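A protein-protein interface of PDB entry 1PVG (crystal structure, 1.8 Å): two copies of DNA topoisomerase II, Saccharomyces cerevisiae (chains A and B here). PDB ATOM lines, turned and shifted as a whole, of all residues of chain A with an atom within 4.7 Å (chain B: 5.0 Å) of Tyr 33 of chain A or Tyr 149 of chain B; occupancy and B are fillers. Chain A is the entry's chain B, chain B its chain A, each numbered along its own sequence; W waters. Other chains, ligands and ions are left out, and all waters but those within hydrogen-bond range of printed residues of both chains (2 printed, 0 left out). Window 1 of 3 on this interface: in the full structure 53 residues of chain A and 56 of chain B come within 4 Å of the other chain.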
ATOM      1  N   HIS A  25     -28.474  20.428  10.043  1.00  0.00           N
ATOM      2  CA  HIS A  25     -27.048  20.185  10.267  1.00  0.00           C
ATOM      3  C   HIS A  25     -26.406  19.374   9.147  1.00  0.00           C
ATOM      4  O   HIS A  25     -25.232  19.570   8.820  1.00  0.00           O
ATOM      5  CB  HIS A  25     -26.790  19.482  11.602  1.00  0.00           C
ATOM      6  CG  HIS A  25     -25.334  19.278  11.886  1.00  0.00           C
ATOM      7  ND1 HIS A  25     -24.737  18.037  11.860  1.00  0.00           N
ATOM      8  CD2 HIS A  25     -24.342  20.167  12.135  1.00  0.00           C
ATOM      9  CE1 HIS A  25     -23.448  18.165  12.116  1.00  0.00           C
ATOM     10  NE2 HIS A  25     -23.182  19.448  12.285  1.00  0.00           N
ATOM     11  N   ILE A  26     -27.171  18.445   8.584  1.00  0.00           N
ATOM     12  CA  ILE A  26     -26.715  17.684   7.433  1.00  0.00           C
ATOM     13  C   ILE A  26     -26.472  18.604   6.231  1.00  0.00           C
ATOM     14  O   ILE A  26     -25.417  18.547   5.604  1.00  0.00           O
ATOM     15  CB  ILE A  26     -27.709  16.520   7.110  1.00  0.00           C
ATOM     16  CG1 ILE A  26     -27.638  15.453   8.213  1.00  0.00           C
ATOM     17  CG2 ILE A  26     -27.397  15.889   5.745  1.00  0.00           C
ATOM     18  CD1 ILE A  26     -28.805  14.455   8.213  1.00  0.00           C
ATOM     19  N   ARG A  29     -23.544  21.138   7.270  1.00  0.00           N
ATOM     20  CA  ARG A  29     -22.258  20.487   7.465  1.00  0.00           C
ATOM     21  C   ARG A  29     -22.277  19.048   6.904  1.00  0.00           C
ATOM     22  O   ARG A  29     -22.296  18.077   7.670  1.00  0.00           O
ATOM     23  CB  ARG A  29     -21.888  20.474   8.963  1.00  0.00           C
ATOM     24  CG  ARG A  29     -21.813  21.848   9.634  1.00  0.00           C
ATOM     25  CD  ARG A  29     -20.445  22.186  10.282  1.00  0.00           C
ATOM     26  NE  ARG A  29     -20.461  23.463  11.021  1.00  0.00           N
ATOM     27  CZ  ARG A  29     -20.696  24.644  10.459  1.00  0.00           C
ATOM     28  NH1 ARG A  29     -20.929  24.719   9.154  1.00  0.00           N
ATOM     29  NH2 ARG A  29     -20.702  25.750  11.193  1.00  0.00           N
ATOM     30  N   PRO A  30     -22.267  18.907   5.576  1.00  0.00           N
ATOM     31  CA  PRO A  30     -22.345  17.579   4.937  1.00  0.00           C
ATOM     32  C   PRO A  30     -21.147  16.659   5.214  1.00  0.00           C
ATOM     33  O   PRO A  30     -21.284  15.450   5.068  1.00  0.00           O
ATOM     34  CB  PRO A  30     -22.401  17.915   3.444  1.00  0.00           C
ATOM     35  CG  PRO A  30     -22.860  19.338   3.392  1.00  0.00           C
ATOM     36  CD  PRO A  30     -22.215  19.988   4.578  1.00  0.00           C
ATOM     37  N   ASP A  31     -20.007  17.224   5.616  1.00  0.00           N
ATOM     38  CA  ASP A  31     -18.734  16.500   5.623  1.00  0.00           C
ATOM     39  C   ASP A  31     -18.706  15.177   6.395  1.00  0.00           C
ATOM     40  O   ASP A  31     -18.223  14.175   5.878  1.00  0.00           O
ATOM     41  CB  ASP A  31     -17.600  17.409   6.087  1.00  0.00           C
ATOM     42  CG  ASP A  31     -17.235  18.436   5.050  1.00  0.00           C
ATOM     43  OD1 ASP A  31     -16.232  18.238   4.350  1.00  0.00           O
ATOM     44  OD2 ASP A  31     -17.911  19.462   4.849  1.00  0.00           O
ATOM     45  N   THR A  32     -19.212  15.168   7.628  1.00  0.00           N
ATOM     46  CA  THR A  32     -19.182  13.933   8.419  1.00  0.00           C
ATOM     47  C   THR A  32     -20.240  12.910   7.979  1.00  0.00           C
ATOM     48  O   THR A  32     -20.154  11.733   8.333  1.00  0.00           O
ATOM     49  CB  THR A  32     -19.272  14.212   9.942  1.00  0.00           C
ATOM     50  OG1 THR A  32     -20.555  14.769  10.264  1.00  0.00           O
ATOM     51  CG2 THR A  32     -18.280  15.300  10.352  1.00  0.00           C
ATOM     52  N   TYR A  33     -21.209  13.349   7.184  1.00  0.00           N
ATOM     53  CA  TYR A  33     -22.237  12.429   6.676  1.00  0.00           C
ATOM     54  C   TYR A  33     -21.893  11.817   5.311  1.00  0.00           C
ATOM     55  O   TYR A  33     -21.990  10.600   5.127  1.00  0.00           O
ATOM     56  CB  TYR A  33     -23.594  13.123   6.619  1.00  0.00           C
ATOM     57  CG  TYR A  33     -24.022  13.738   7.934  1.00  0.00           C
ATOM     58  CD1 TYR A  33     -24.661  12.968   8.914  1.00  0.00           C
ATOM     59  CD2 TYR A  33     -23.797  15.088   8.197  1.00  0.00           C
ATOM     60  CE1 TYR A  33     -25.065  13.538  10.124  1.00  0.00           C
ATOM     61  CE2 TYR A  33     -24.200  15.668   9.390  1.00  0.00           C
ATOM     62  CZ  TYR A  33     -24.834  14.885  10.352  1.00  0.00           C
ATOM     63  OH  TYR A  33     -25.227  15.456  11.541  1.00  0.00           O
ATOM     64  N   ILE A  34     -21.504  12.657   4.351  1.00  0.00           N
ATOM     65  CA  ILE A  34     -21.290  12.193   2.967  1.00  0.00           C
ATOM     66  C   ILE A  34     -19.903  12.539   2.410  1.00  0.00           C
ATOM     67  O   ILE A  34     -19.568  12.163   1.285  1.00  0.00           O
ATOM     68  CB  ILE A  34     -22.405  12.733   2.002  1.00  0.00           C
ATOM     69  CG1 ILE A  34     -22.370  14.271   1.931  1.00  0.00           C
ATOM     70  CG2 ILE A  34     -23.785  12.174   2.387  1.00  0.00           C
ATOM     71  CD1 ILE A  34     -23.195  14.873   0.793  1.00  0.00           C
ATOM     72  N   GLY A  35     -19.097  13.240   3.198  1.00  0.00           N
ATOM     73  CA  GLY A  35     -17.827  13.750   2.721  1.00  0.00           C
ATOM     74  C   GLY A  35     -17.986  15.160   2.191  1.00  0.00           C
ATOM     75  O   GLY A  35     -19.069  15.742   2.273  1.00  0.00           O
ATOM     76  N   TYR A 149     -28.705   5.891   7.990  1.00  0.00           N
ATOM     77  CA  TYR A 149     -28.574   7.203   7.345  1.00  0.00           C
ATOM     78  C   TYR A 149     -28.549   7.135   5.812  1.00  0.00           C
ATOM     79  O   TYR A 149     -29.129   7.986   5.147  1.00  0.00           O
ATOM     80  CB  TYR A 149     -27.277   7.888   7.801  1.00  0.00           C
ATOM     81  CG  TYR A 149     -27.369   8.626   9.109  1.00  0.00           C
ATOM     82  CD1 TYR A 149     -26.609   8.225  10.205  1.00  0.00           C
ATOM     83  CD2 TYR A 149     -28.182   9.747   9.243  1.00  0.00           C
ATOM     84  CE1 TYR A 149     -26.671   8.906  11.413  1.00  0.00           C
ATOM     85  CE2 TYR A 149     -28.264  10.437  10.447  1.00  0.00           C
ATOM     86  CZ  TYR A 149     -27.508  10.015  11.526  1.00  0.00           C
ATOM     87  OH  TYR A 149     -27.568  10.701  12.719  1.00  0.00           O
ATOM     88  N   LEU A 153     -29.715  10.173   3.395  1.00  0.00           N
ATOM     89  CA  LEU A 153     -28.697  11.119   2.939  1.00  0.00           C
ATOM     90  C   LEU A 153     -28.779  11.342   1.423  1.00  0.00           C
ATOM     91  O   LEU A 153     -28.650  12.464   0.943  1.00  0.00           O
ATOM     92  CB  LEU A 153     -27.295  10.642   3.338  1.00  0.00           C
ATOM     93  CG  LEU A 153     -27.001  10.693   4.841  1.00  0.00           C
ATOM     94  CD1 LEU A 153     -25.613  10.147   5.139  1.00  0.00           C
ATOM     95  CD2 LEU A 153     -27.154  12.111   5.384  1.00  0.00           C
ATOM     96  N   GLN A 370     -19.730   8.092   8.924  1.00  0.00           N
ATOM     97  CA  GLN A 370     -20.808   7.562   8.085  1.00  0.00           C
ATOM     98  C   GLN A 370     -20.328   7.177   6.675  1.00  0.00           C
ATOM     99  O   GLN A 370     -20.889   6.281   6.054  1.00  0.00           O
ATOM    100  CB  GLN A 370     -21.963   8.571   8.012  1.00  0.00           C
ATOM    101  CG  GLN A 370     -23.118   8.188   7.066  1.00  0.00           C
ATOM    102  CD  GLN A 370     -23.778   6.878   7.448  1.00  0.00           C
ATOM    103  OE1 GLN A 370     -23.798   6.505   8.622  1.00  0.00           O
ATOM    104  NE2 GLN A 370     -24.315   6.174   6.461  1.00  0.00           N
ATOM    105  N   THR A 371     -19.298   7.854   6.169  1.00  0.00           N
ATOM    106  CA  THR A 371     -18.805   7.544   4.822  1.00  0.00           C
ATOM    107  C   THR A 371     -18.170   6.162   4.755  1.00  0.00           C
ATOM    108  O   THR A 371     -17.992   5.615   3.672  1.00  0.00           O
ATOM    109  CB  THR A 371     -17.798   8.591   4.321  1.00  0.00           C
ATOM    110  OG1 THR A 371     -16.635   8.572   5.155  1.00  0.00           O
ATOM    111  CG2 THR A 371     -18.360  10.002   4.470  1.00  0.00           C
ATOM    112  N   GLN B  22     -32.001  10.553  18.056  1.00  0.00           N
ATOM    113  CA  GLN B  22     -30.609  10.949  17.964  1.00  0.00           C
ATOM    114  C   GLN B  22     -29.868  10.604  19.250  1.00  0.00           C
ATOM    115  O   GLN B  22     -28.737  10.107  19.210  1.00  0.00           O
ATOM    116  CB  GLN B  22     -30.499  12.440  17.689  1.00  0.00           C
ATOM    117  CG  GLN B  22     -29.073  12.939  17.652  1.00  0.00           C
ATOM    118  CD  GLN B  22     -28.945  14.234  16.907  1.00  0.00           C
ATOM    119  OE1 GLN B  22     -29.897  15.036  16.862  1.00  0.00           O
ATOM    120  NE2 GLN B  22     -27.796  14.442  16.295  1.00  0.00           N
ATOM    121  N   ILE B  26     -26.649   7.926  19.665  1.00  0.00           N
ATOM    122  CA  ILE B  26     -25.353   8.282  20.237  1.00  0.00           C
ATOM    123  C   ILE B  26     -24.921   7.222  21.260  1.00  0.00           C
ATOM    124  O   ILE B  26     -23.781   6.766  21.246  1.00  0.00           O
ATOM    125  CB  ILE B  26     -25.406   9.693  20.876  1.00  0.00           C
ATOM    126  CG1 ILE B  26     -25.563  10.759  19.782  1.00  0.00           C
ATOM    127  CG2 ILE B  26     -24.151   9.969  21.707  1.00  0.00           C
ATOM    128  CD1 ILE B  26     -25.973  12.135  20.308  1.00  0.00           C
ATOM    129  N   TYR B  33     -19.364   9.605  16.943  1.00  0.00           N
ATOM    130  CA  TYR B  33     -19.506  10.783  17.815  1.00  0.00           C
ATOM    131  C   TYR B  33     -18.282  11.012  18.699  1.00  0.00           C
ATOM    132  O   TYR B  33     -17.735  12.112  18.730  1.00  0.00           O
ATOM    133  CB  TYR B  33     -20.772  10.684  18.675  1.00  0.00           C
ATOM    134  CG  TYR B  33     -22.053  10.488  17.882  1.00  0.00           C
ATOM    135  CD1 TYR B  33     -22.723  11.575  17.320  1.00  0.00           C
ATOM    136  CD2 TYR B  33     -22.604   9.218  17.711  1.00  0.00           C
ATOM    137  CE1 TYR B  33     -23.909  11.402  16.594  1.00  0.00           C
ATOM    138  CE2 TYR B  33     -23.784   9.030  16.976  1.00  0.00           C
ATOM    139  CZ  TYR B  33     -24.432  10.130  16.430  1.00  0.00           C
ATOM    140  OH  TYR B  33     -25.601   9.954  15.714  1.00  0.00           O
ATOM    141  N   LEU B 129     -28.734  18.873  22.056  1.00  0.00           N
ATOM    142  CA  LEU B 129     -27.902  18.576  20.895  1.00  0.00           C
ATOM    143  C   LEU B 129     -28.044  19.660  19.843  1.00  0.00           C
ATOM    144  O   LEU B 129     -29.086  20.309  19.757  1.00  0.00           O
ATOM    145  CB  LEU B 129     -28.294  17.221  20.289  1.00  0.00           C
ATOM    146  CG  LEU B 129     -27.918  16.011  21.143  1.00  0.00           C
ATOM    147  CD1 LEU B 129     -28.574  14.767  20.579  1.00  0.00           C
ATOM    148  CD2 LEU B 129     -26.407  15.852  21.205  1.00  0.00           C
ATOM    149  N   LEU B 130     -26.987  19.856  19.059  1.00  0.00           N
ATOM    150  CA  LEU B 130     -27.029  20.743  17.890  1.00  0.00           C
ATOM    151  C   LEU B 130     -27.249  22.212  18.284  1.00  0.00           C
ATOM    152  O   LEU B 130     -28.086  22.924  17.710  1.00  0.00           O
ATOM    153  CB  LEU B 130     -28.069  20.245  16.869  1.00  0.00           C
ATOM    154  CG  LEU B 130     -27.678  18.906  16.214  1.00  0.00           C
ATOM    155  CD1 LEU B 130     -28.867  18.257  15.493  1.00  0.00           C
ATOM    156  CD2 LEU B 130     -26.499  19.097  15.251  1.00  0.00           C
ATOM    157  N   THR B 131     -26.472  22.644  19.273  1.00  0.00           N
ATOM    158  CA  THR B 131     -26.488  24.016  19.757  1.00  0.00           C
ATOM    159  C   THR B 131     -25.063  24.541  19.785  1.00  0.00           C
ATOM    160  O   THR B 131     -24.155  23.881  20.316  1.00  0.00           O
ATOM    161  CB  THR B 131     -27.097  24.090  21.169  1.00  0.00           C
ATOM    162  OG1 THR B 131     -26.458  23.130  22.017  1.00  0.00           O
ATOM    163  CG2 THR B 131     -28.570  23.658  21.160  1.00  0.00           C
ATOM    164  N   ASN B 147     -19.524  21.924  15.379  1.00  0.00           N
ATOM    165  CA  ASN B 147     -20.772  21.188  15.142  1.00  0.00           C
ATOM    166  C   ASN B 147     -21.881  21.314  16.170  1.00  0.00           C
ATOM    167  O   ASN B 147     -23.022  20.936  15.893  1.00  0.00           O
ATOM    168  CB  ASN B 147     -20.480  19.713  14.930  1.00  0.00           C
ATOM    169  CG  ASN B 147     -19.586  19.476  13.759  1.00  0.00           C
ATOM    170  OD1 ASN B 147     -19.930  19.816  12.628  1.00  0.00           O
ATOM    171  ND2 ASN B 147     -18.413  18.915  14.016  1.00  0.00           N
ATOM    172  N   GLY B 148     -21.545  21.785  17.358  1.00  0.00           N
ATOM    173  CA  GLY B 148     -22.534  21.926  18.416  1.00  0.00           C
ATOM    174  C   GLY B 148     -22.910  20.619  19.090  1.00  0.00           C
ATOM    175  O   GLY B 148     -24.051  20.458  19.528  1.00  0.00           O
ATOM    176  N   TYR B 149     -21.944  19.695  19.186  1.00  0.00           N
ATOM    177  CA  TYR B 149     -22.133  18.399  19.846  1.00  0.00           C
ATOM    178  C   TYR B 149     -21.279  18.232  21.100  1.00  0.00           C
ATOM    179  O   TYR B 149     -21.726  17.650  22.081  1.00  0.00           O
ATOM    180  CB  TYR B 149     -21.752  17.262  18.895  1.00  0.00           C
ATOM    181  CG  TYR B 149     -22.854  16.812  17.979  1.00  0.00           C
ATOM    182  CD1 TYR B 149     -22.836  17.152  16.627  1.00  0.00           C
ATOM    183  CD2 TYR B 149     -23.904  16.023  18.451  1.00  0.00           C
ATOM    184  CE1 TYR B 149     -23.838  16.728  15.768  1.00  0.00           C
ATOM    185  CE2 TYR B 149     -24.913  15.593  17.600  1.00  0.00           C
ATOM    186  CZ  TYR B 149     -24.874  15.958  16.257  1.00  0.00           C
ATOM    187  OH  TYR B 149     -25.868  15.545  15.399  1.00  0.00           O
ATOM    188  N   GLY B 150     -20.045  18.737  21.048  1.00  0.00           N
ATOM    189  CA  GLY B 150     -18.999  18.365  21.988  1.00  0.00           C
ATOM    190  C   GLY B 150     -19.364  18.316  23.464  1.00  0.00           C
ATOM    191  O   GLY B 150     -19.117  17.304  24.127  1.00  0.00           O
ATOM    192  N   ALA B 151     -19.918  19.419  23.977  1.00  0.00           N
ATOM    193  CA  ALA B 151     -20.291  19.535  25.393  1.00  0.00           C
ATOM    194  C   ALA B 151     -21.420  18.561  25.753  1.00  0.00           C
ATOM    195  O   ALA B 151     -21.442  17.991  26.852  1.00  0.00           O
ATOM    196  CB  ALA B 151     -20.697  20.969  25.715  1.00  0.00           C
ATOM    197  N   LYS B 152     -22.340  18.361  24.817  1.00  0.00           N
ATOM    198  CA  LYS B 152     -23.472  17.466  25.032  1.00  0.00           C
ATOM    199  C   LYS B 152     -23.032  16.013  25.001  1.00  0.00           C
ATOM    200  O   LYS B 152     -23.554  15.180  25.746  1.00  0.00           O
ATOM    201  CB  LYS B 152     -24.577  17.704  23.988  1.00  0.00           C
ATOM    202  CG  LYS B 152     -25.529  18.867  24.324  1.00  0.00           C
ATOM    203  CD  LYS B 152     -24.844  20.233  24.148  1.00  0.00           C
ATOM    204  CE  LYS B 152     -24.393  20.467  22.683  1.00  0.00           C
ATOM    205  NZ  LYS B 152     -23.849  21.849  22.492  1.00  0.00           N
ATOM    206  N   LEU B 153     -22.079  15.699  24.130  1.00  0.00           N
ATOM    207  CA  LEU B 153     -21.524  14.349  24.108  1.00  0.00           C
ATOM    208  C   LEU B 153     -20.895  14.000  25.450  1.00  0.00           C
ATOM    209  O   LEU B 153     -21.115  12.910  25.976  1.00  0.00           O
ATOM    210  CB  LEU B 153     -20.540  14.172  22.954  1.00  0.00           C
ATOM    211  CG  LEU B 153     -21.200  14.303  21.575  1.00  0.00           C
ATOM    212  CD1 LEU B 153     -20.158  14.276  20.460  1.00  0.00           C
ATOM    213  CD2 LEU B 153     -22.272  13.197  21.375  1.00  0.00           C
ATOM    214  N   GLN B 370     -16.782  13.929  13.865  1.00  0.00           N
ATOM    215  CA  GLN B 370     -16.904  14.730  15.086  1.00  0.00           C
ATOM    216  C   GLN B 370     -15.645  14.680  15.963  1.00  0.00           C
ATOM    217  O   GLN B 370     -15.347  15.647  16.673  1.00  0.00           O
ATOM    218  CB  GLN B 370     -18.134  14.305  15.894  1.00  0.00           C
ATOM    219  CG  GLN B 370     -18.282  15.005  17.269  1.00  0.00           C
ATOM    220  CD  GLN B 370     -18.463  16.506  17.166  1.00  0.00           C
ATOM    221  OE1 GLN B 370     -19.051  16.996  16.210  1.00  0.00           O
ATOM    222  NE2 GLN B 370     -17.975  17.242  18.171  1.00  0.00           N
HETATM  223  O   HOH W   1     -23.964  13.762  13.437  1.00  0.00           O
HETATM  224  O   HOH W   2     -24.617  11.085  13.201  1.00  0.00           O
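Leu 130 of chain B touches His 25 of chain A. CE1 of Tyr 149 of chain B touches CE1 of His 25 of chain A, at 3.9 Å. Arg 29 of chain A touches Asn 147 of chain B. Tyr 33 of chain A touches Tyr 149 of chain B. OH of Tyr 33 of chain B touches OH of Tyr 149 of chain A (3.7 Å).
Tyr 33 of chain A touches Tyr 149 of chain B, and with the chains exchanged Tyr 149 of chain A touches Tyr 33 of chain B. Positions printed for both chains: 26, 33, 149, 153 and 370.
Water W1 bridges the side-chain hydroxyl (OH) of Tyr 33 of chain A (2.8 Å) and the side-chain hydroxyl (OH) of Tyr 149 of chain B (3.3 Å). Water W2 lies within hydrogen-bond range of OH of Tyr 33 of chain B (2.9 Å) and OH of Tyr 149 of chain A (3.0 Å).
Tyr 33 of chain A touches just one residue of chain B: Tyr 149. Tyr 149 of chain B touches just these residues of chain A: His 25 (3.9 Å) and Tyr 33 (3.9 Å). Printed residues of chain A within 4 Å of Leu 130 of chain B: His 25 (3.6 Å). Printed residues of chain A within 4 Å of Tyr 33 of chain B: Tyr 149 (3.7 Å). Of the printed residues of chain B, His 25 of chain A touches Leu 130 (3.6 Å), Asn 147 (3.3 Å) and Tyr 149 (3.9 Å). Leu 129 of chain B touches none of the printed residues of chain A. The nearest printed residue of chain A that does not touch Tyr 149 of chain B is Tyr 149 of chain A (5.8 Å).
A ring nitrogen (NE2) of His 25 of chain A sits at hydrogen-bond distance from the side-chain amide oxygen (OD1) of Asn 147 of chain B, at 3.3 Å.
The side-chain amide nitrogen of Asn 147 of chain B sits at hydrogen-bond distance from the side-chain amide oxygen of Gln 370 of chain B. A ring nitrogen (ND1) of His 25 of chain A sits at hydrogen-bond distance from the side-chain hydroxyl of Tyr 33 of chain A (2.6 Å). The backbone NH of Leu 130 of chain B is in hydrogen-bond range of the backbone carbonyl oxygen of Gly 148 of chain B (3.0 Å).
Printed residues of chain A that touch a printed residue of chain B: His 25, Arg 29, Tyr 33 and Tyr 149. Hydrophobic or aromatic side chains of chain A within 4 Å of the printed part of chain B: His 25, Tyr 33 and Tyr 149. Among the printed residues, 6 pairs touch across the chains. Among the printed residues, no Asp or Glu carboxylate lies within 4 Å of a Lys or Arg side-chain nitrogen of the other chain.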
